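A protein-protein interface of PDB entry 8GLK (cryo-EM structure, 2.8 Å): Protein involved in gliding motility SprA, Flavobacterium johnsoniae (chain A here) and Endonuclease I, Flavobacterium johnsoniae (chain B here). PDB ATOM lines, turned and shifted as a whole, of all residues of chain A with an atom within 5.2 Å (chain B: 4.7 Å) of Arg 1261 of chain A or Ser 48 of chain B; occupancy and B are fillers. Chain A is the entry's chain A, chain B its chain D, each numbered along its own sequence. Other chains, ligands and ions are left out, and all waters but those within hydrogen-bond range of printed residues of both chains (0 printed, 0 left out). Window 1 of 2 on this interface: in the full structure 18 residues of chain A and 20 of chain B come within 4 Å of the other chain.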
ATOM      1  N   SER A 864      13.221 -18.934   0.808  1.00  0.00           N
ATOM      2  CA  SER A 864      12.200 -18.826   1.836  1.00  0.00           C
ATOM      3  C   SER A 864      12.572 -17.750   2.851  1.00  0.00           C
ATOM      4  O   SER A 864      13.668 -17.184   2.830  1.00  0.00           O
ATOM      5  CB  SER A 864      12.000 -20.171   2.533  1.00  0.00           C
ATOM      6  OG  SER A 864      13.211 -20.647   3.091  1.00  0.00           O
ATOM      7  N   GLN A 865      11.628 -17.466   3.749  1.00  0.00           N
ATOM      8  CA  GLN A 865      11.840 -16.566   4.882  1.00  0.00           C
ATOM      9  C   GLN A 865      12.244 -15.162   4.425  1.00  0.00           C
ATOM     10  O   GLN A 865      13.344 -14.680   4.696  1.00  0.00           O
ATOM     11  CB  GLN A 865      12.874 -17.149   5.849  1.00  0.00           C
ATOM     12  CG  GLN A 865      12.427 -18.436   6.509  1.00  0.00           C
ATOM     13  CD  GLN A 865      12.012 -18.229   7.948  1.00  0.00           C
ATOM     14  OE1 GLN A 865      12.715 -17.578   8.717  1.00  0.00           O
ATOM     15  NE2 GLN A 865      10.865 -18.783   8.320  1.00  0.00           N
ATOM     16  N   SER A 866      11.327 -14.511   3.716  1.00  0.00           N
ATOM     17  CA  SER A 866      11.490 -13.096   3.431  1.00  0.00           C
ATOM     18  C   SER A 866      11.154 -12.272   4.673  1.00  0.00           C
ATOM     19  O   SER A 866      10.494 -12.740   5.605  1.00  0.00           O
ATOM     20  CB  SER A 866      10.614 -12.676   2.250  1.00  0.00           C
ATOM     21  OG  SER A 866       9.274 -13.086   2.431  1.00  0.00           O
ATOM     22  N   THR A 867      11.636 -11.033   4.687  1.00  0.00           N
ATOM     23  CA  THR A 867      11.533 -10.179   5.861  1.00  0.00           C
ATOM     24  C   THR A 867      10.896  -8.846   5.497  1.00  0.00           C
ATOM     25  O   THR A 867      10.995  -8.382   4.359  1.00  0.00           O
ATOM     26  CB  THR A 867      12.910  -9.928   6.495  1.00  0.00           C
ATOM     27  OG1 THR A 867      13.838  -9.524   5.481  1.00  0.00           O
ATOM     28  CG2 THR A 867      13.427 -11.190   7.164  1.00  0.00           C
ATOM     29  N   ILE A 868      10.234  -8.241   6.478  1.00  0.00           N
ATOM     30  CA  ILE A 868       9.704  -6.887   6.366  1.00  0.00           C
ATOM     31  C   ILE A 868      10.335  -6.065   7.481  1.00  0.00           C
ATOM     32  O   ILE A 868      10.183  -6.397   8.663  1.00  0.00           O
ATOM     33  CB  ILE A 868       8.171  -6.862   6.460  1.00  0.00           C
ATOM     34  CG1 ILE A 868       7.565  -7.876   5.490  1.00  0.00           C
ATOM     35  CG2 ILE A 868       7.646  -5.477   6.138  1.00  0.00           C
ATOM     36  CD1 ILE A 868       6.093  -8.127   5.715  1.00  0.00           C
ATOM     37  N   GLY A1002       0.010 -13.779   3.812  1.00  0.00           N
ATOM     38  CA  GLY A1002       1.439 -13.576   3.688  1.00  0.00           C
ATOM     39  C   GLY A1002       2.289 -14.583   4.423  1.00  0.00           C
ATOM     40  O   GLY A1002       3.508 -14.599   4.231  1.00  0.00           O
ATOM     41  N   ASN A1003       1.670 -15.426   5.251  1.00  0.00           N
ATOM     42  CA  ASN A1003       2.376 -16.433   6.042  1.00  0.00           C
ATOM     43  C   ASN A1003       3.459 -15.795   6.910  1.00  0.00           C
ATOM     44  O   ASN A1003       4.583 -16.292   6.997  1.00  0.00           O
ATOM     45  CB  ASN A1003       2.964 -17.529   5.150  1.00  0.00           C
ATOM     46  CG  ASN A1003       3.316 -18.786   5.921  1.00  0.00           C
ATOM     47  OD1 ASN A1003       2.705 -19.093   6.942  1.00  0.00           O
ATOM     48  ND2 ASN A1003       4.311 -19.518   5.438  1.00  0.00           N
ATOM     49  N   VAL A1004       3.121 -14.679   7.553  1.00  0.00           N
ATOM     50  CA  VAL A1004       4.032 -14.028   8.486  1.00  0.00           C
ATOM     51  C   VAL A1004       4.277 -14.983   9.643  1.00  0.00           C
ATOM     52  O   VAL A1004       3.368 -15.271  10.430  1.00  0.00           O
ATOM     53  CB  VAL A1004       3.479 -12.680   8.978  1.00  0.00           C
ATOM     54  CG1 VAL A1004       4.372 -12.108  10.066  1.00  0.00           C
ATOM     55  CG2 VAL A1004       3.356 -11.707   7.819  1.00  0.00           C
ATOM     56  N   GLU A1005       5.506 -15.483   9.756  1.00  0.00           N
ATOM     57  CA  GLU A1005       5.757 -16.595  10.661  1.00  0.00           C
ATOM     58  C   GLU A1005       6.223 -16.149  12.040  1.00  0.00           C
ATOM     59  O   GLU A1005       5.770 -16.709  13.044  1.00  0.00           O
ATOM     60  CB  GLU A1005       6.777 -17.554  10.045  1.00  0.00           C
ATOM     61  CG  GLU A1005       6.208 -18.401   8.916  1.00  0.00           C
ATOM     62  CD  GLU A1005       5.306 -19.525   9.402  1.00  0.00           C
ATOM     63  OE1 GLU A1005       4.278 -19.244  10.050  1.00  0.00           O
ATOM     64  OE2 GLU A1005       5.620 -20.698   9.119  1.00  0.00           O
ATOM     65  N   LEU A1259       9.577  -8.485  10.588  1.00  0.00           N
ATOM     66  CA  LEU A1259       8.501  -9.466  10.537  1.00  0.00           C
ATOM     67  C   LEU A1259       8.875 -10.474   9.458  1.00  0.00           C
ATOM     68  O   LEU A1259       8.955 -10.124   8.278  1.00  0.00           O
ATOM     69  CB  LEU A1259       7.164  -8.797  10.233  1.00  0.00           C
ATOM     70  CG  LEU A1259       6.515  -7.985  11.354  1.00  0.00           C
ATOM     71  CD1 LEU A1259       5.300  -7.236  10.836  1.00  0.00           C
ATOM     72  CD2 LEU A1259       6.132  -8.886  12.510  1.00  0.00           C
ATOM     73  N   VAL A1260       9.141 -11.713   9.861  1.00  0.00           N
ATOM     74  CA  VAL A1260       9.630 -12.743   8.956  1.00  0.00           C
ATOM     75  C   VAL A1260       8.465 -13.622   8.532  1.00  0.00           C
ATOM     76  O   VAL A1260       7.753 -14.182   9.380  1.00  0.00           O
ATOM     77  CB  VAL A1260      10.738 -13.582   9.612  1.00  0.00           C
ATOM     78  CG1 VAL A1260      11.275 -14.605   8.626  1.00  0.00           C
ATOM     79  CG2 VAL A1260      11.849 -12.681  10.106  1.00  0.00           C
ATOM     80  N   ARG A1261       8.281 -13.740   7.217  1.00  0.00           N
ATOM     81  CA  ARG A1261       7.256 -14.567   6.604  1.00  0.00           C
ATOM     82  C   ARG A1261       7.916 -15.644   5.751  1.00  0.00           C
ATOM     83  O   ARG A1261       8.942 -15.406   5.104  1.00  0.00           O
ATOM     84  CB  ARG A1261       6.298 -13.711   5.760  1.00  0.00           C
ATOM     85  CG  ARG A1261       6.897 -13.155   4.481  1.00  0.00           C
ATOM     86  CD  ARG A1261       6.015 -12.076   3.872  1.00  0.00           C
ATOM     87  NE  ARG A1261       5.163 -12.591   2.808  1.00  0.00           N
ATOM     88  CZ  ARG A1261       5.510 -12.643   1.529  1.00  0.00           C
ATOM     89  NH1 ARG A1261       6.690 -12.212   1.116  1.00  0.00           N
ATOM     90  NH2 ARG A1261       4.649 -13.135   0.643  1.00  0.00           N
ATOM     91  N   GLY A1262       7.335 -16.839   5.773  1.00  0.00           N
ATOM     92  CA  GLY A1262       7.936 -17.967   5.089  1.00  0.00           C
ATOM     93  C   GLY A1262       7.133 -18.515   3.928  1.00  0.00           C
ATOM     94  O   GLY A1262       5.916 -18.325   3.854  1.00  0.00           O
ATOM     95  N   GLU A1263       7.816 -19.197   3.006  1.00  0.00           N
ATOM     96  CA  GLU A1263       7.136 -19.872   1.907  1.00  0.00           C
ATOM     97  C   GLU A1263       6.494 -21.179   2.348  1.00  0.00           C
ATOM     98  O   GLU A1263       5.446 -21.559   1.816  1.00  0.00           O
ATOM     99  CB  GLU A1263       8.114 -20.136   0.760  1.00  0.00           C
ATOM    100  CG  GLU A1263       8.634 -18.886   0.075  1.00  0.00           C
ATOM    101  CD  GLU A1263       7.548 -18.136  -0.672  1.00  0.00           C
ATOM    102  OE1 GLU A1263       6.609 -18.791  -1.175  1.00  0.00           O
ATOM    103  OE2 GLU A1263       7.632 -16.894  -0.761  1.00  0.00           O
ATOM    104  N   GLY B  11      12.919  -4.032  -0.328  1.00  0.00           N
ATOM    105  CA  GLY B  11      12.504  -5.205  -1.070  1.00  0.00           C
ATOM    106  C   GLY B  11      10.999  -5.241  -1.232  1.00  0.00           C
ATOM    107  O   GLY B  11      10.472  -5.895  -2.134  1.00  0.00           O
ATOM    108  N   ASN B  12      10.302  -4.534  -0.349  1.00  0.00           N
ATOM    109  CA  ASN B  12       8.850  -4.416  -0.406  1.00  0.00           C
ATOM    110  C   ASN B  12       8.512  -3.040  -0.966  1.00  0.00           C
ATOM    111  O   ASN B  12       8.812  -2.020  -0.338  1.00  0.00           O
ATOM    112  CB  ASN B  12       8.242  -4.607   0.981  1.00  0.00           C
ATOM    113  CG  ASN B  12       8.489  -5.993   1.544  1.00  0.00           C
ATOM    114  OD1 ASN B  12       7.995  -6.988   1.014  1.00  0.00           O
ATOM    115  ND2 ASN B  12       9.260  -6.064   2.619  1.00  0.00           N
ATOM    116  N   ILE B  46       1.335  -4.198  -4.408  1.00  0.00           N
ATOM    117  CA  ILE B  46       2.479  -4.454  -3.542  1.00  0.00           C
ATOM    118  C   ILE B  46       3.307  -5.603  -4.105  1.00  0.00           C
ATOM    119  O   ILE B  46       2.772  -6.641  -4.515  1.00  0.00           O
ATOM    120  CB  ILE B  46       2.018  -4.728  -2.101  1.00  0.00           C
ATOM    121  CG1 ILE B  46       3.223  -4.823  -1.161  1.00  0.00           C
ATOM    122  CG2 ILE B  46       1.150  -5.977  -2.019  1.00  0.00           C
ATOM    123  CD1 ILE B  46       2.868  -4.667   0.301  1.00  0.00           C
ATOM    124  N   ILE B  47       4.618  -5.404  -4.155  1.00  0.00           N
ATOM    125  CA  ILE B  47       5.570  -6.384  -4.658  1.00  0.00           C
ATOM    126  C   ILE B  47       6.538  -6.679  -3.520  1.00  0.00           C
ATOM    127  O   ILE B  47       7.142  -5.763  -2.944  1.00  0.00           O
ATOM    128  CB  ILE B  47       6.303  -5.883  -5.907  1.00  0.00           C
ATOM    129  CG1 ILE B  47       5.299  -5.562  -7.016  1.00  0.00           C
ATOM    130  CG2 ILE B  47       7.313  -6.915  -6.382  1.00  0.00           C
ATOM    131  CD1 ILE B  47       4.482  -6.753  -7.461  1.00  0.00           C
ATOM    132  N   SER B  48       6.683  -7.963  -3.195  1.00  0.00           N
ATOM    133  CA  SER B  48       7.510  -8.424  -2.083  1.00  0.00           C
ATOM    134  C   SER B  48       8.657  -9.255  -2.647  1.00  0.00           C
ATOM    135  O   SER B  48       8.495 -10.444  -2.937  1.00  0.00           O
ATOM    136  CB  SER B  48       6.679  -9.229  -1.089  1.00  0.00           C
ATOM    137  OG  SER B  48       5.637  -8.443  -0.539  1.00  0.00           O
ATOM    138  N   VAL B  49       9.821  -8.626  -2.800  1.00  0.00           N
ATOM    139  CA  VAL B  49      11.016  -9.307  -3.284  1.00  0.00           C
ATOM    140  C   VAL B  49      12.144  -9.100  -2.281  1.00  0.00           C
ATOM    141  O   VAL B  49      13.324  -9.071  -2.649  1.00  0.00           O
ATOM    142  CB  VAL B  49      11.415  -8.820  -4.691  1.00  0.00           C
ATOM    143  CG1 VAL B  49      10.314  -9.136  -5.688  1.00  0.00           C
ATOM    144  CG2 VAL B  49      11.708  -7.326  -4.684  1.00  0.00           C
ATOM    145  N   SER B  50      11.788  -8.969  -1.006  1.00  0.00           N
ATOM    146  CA  SER B  50      12.752  -8.682   0.056  1.00  0.00           C
ATOM    147  C   SER B  50      13.709  -9.836   0.336  1.00  0.00           C
ATOM    148  O   SER B  50      14.541  -9.703   1.244  1.00  0.00           O
ATOM    149  CB  SER B  50      12.009  -8.301   1.336  1.00  0.00           C
ATOM    150  OG  SER B  50      11.271  -9.399   1.841  1.00  0.00           O
ATOM    151  N   TYR B  51      13.636 -10.949  -0.386  1.00  0.00           N
ATOM    152  CA  TYR B  51      14.613 -12.022  -0.257  1.00  0.00           C
ATOM    153  C   TYR B  51      15.841 -11.799  -1.128  1.00  0.00           C
ATOM    154  O   TYR B  51      16.821 -12.538  -0.994  1.00  0.00           O
ATOM    155  CB  TYR B  51      13.972 -13.371  -0.603  1.00  0.00           C
ATOM    156  CG  TYR B  51      12.988 -13.319  -1.752  1.00  0.00           C
ATOM    157  CD1 TYR B  51      11.643 -13.048  -1.531  1.00  0.00           C
ATOM    158  CD2 TYR B  51      13.404 -13.540  -3.057  1.00  0.00           C
ATOM    159  CE1 TYR B  51      10.743 -12.999  -2.578  1.00  0.00           C
ATOM    160  CE2 TYR B  51      12.510 -13.493  -4.111  1.00  0.00           C
ATOM    161  CZ  TYR B  51      11.181 -13.223  -3.866  1.00  0.00           C
ATOM    162  OH  TYR B  51      10.287 -13.175  -4.911  1.00  0.00           O
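The side-chain hydroxyl (OG) of Ser 50 of chain B is in hydrogen-bond range of the backbone carbonyl oxygen (O) of Thr 867 of chain A (2.7 Å).
The side-chain amide nitrogen of Asn 12 of chain B lies within hydrogen-bond range of the backbone carbonyl oxygen of Thr 867 of chain A (3.4 Å).
The backbone carbonyl oxygen (O) of Arg 1261 of chain A lies within hydrogen-bond range of the backbone NH (N) of Ser 866 of chain A.
The backbone carbonyl oxygen (O) of Gly 1002 of chain A sits at hydrogen-bond distance from the guanidinium group (NE) of Arg 1261 of chain A (3.0 Å).
N of Ile 868 of chain A is in hydrogen-bond range of O of Leu 1259 of chain A, at 2.9 Å.
OD1 of Asn 12 of chain B sits at hydrogen-bond distance from OG of Ser 48 of chain B (3.2 Å).
Among the printed residues, pairs that only touch across the chains: Ser 866 of chain A with Ser 50 of chain B, Arg 1261 of chain A with Ser 48 of chain B, Ile 868 of chain A with Asn 12 of chain B and Ser 866 of chain A with Tyr 51 of chain B.
Printed residues of chain B within 4 Å of Ser 866 of chain A: Ser 50 and Tyr 51.
Printed residues of chain B within 4 Å of Ile 868 of chain A: Asn 12 (3.8 Å).
Val 1260 of chain A touches none of the printed residues of chain B.
Of chain A, only Arg 1261 comes within 4 Å of Ser 48 of chain B.
The nearest printed residue of chain B that does not touch Arg 1261 of chain A is Asn 12 of chain B (5.4 Å).
The nearest printed residue of chain B that does not touch Ser 866 of chain A is Ser 48 of chain B (5.8 Å).
Of the 8 printed residues of chain B, 4 touch a printed residue of chain A.
Printed residues of chain B that touch a printed residue of chain A: Asn 12, Ser 48, Ser 50 and Tyr 51.
Hydrophobic or aromatic side chains of chain A that line the printed part of chain B: Ile 868.
Among the printed residues, 6 pairs touch across the chains.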
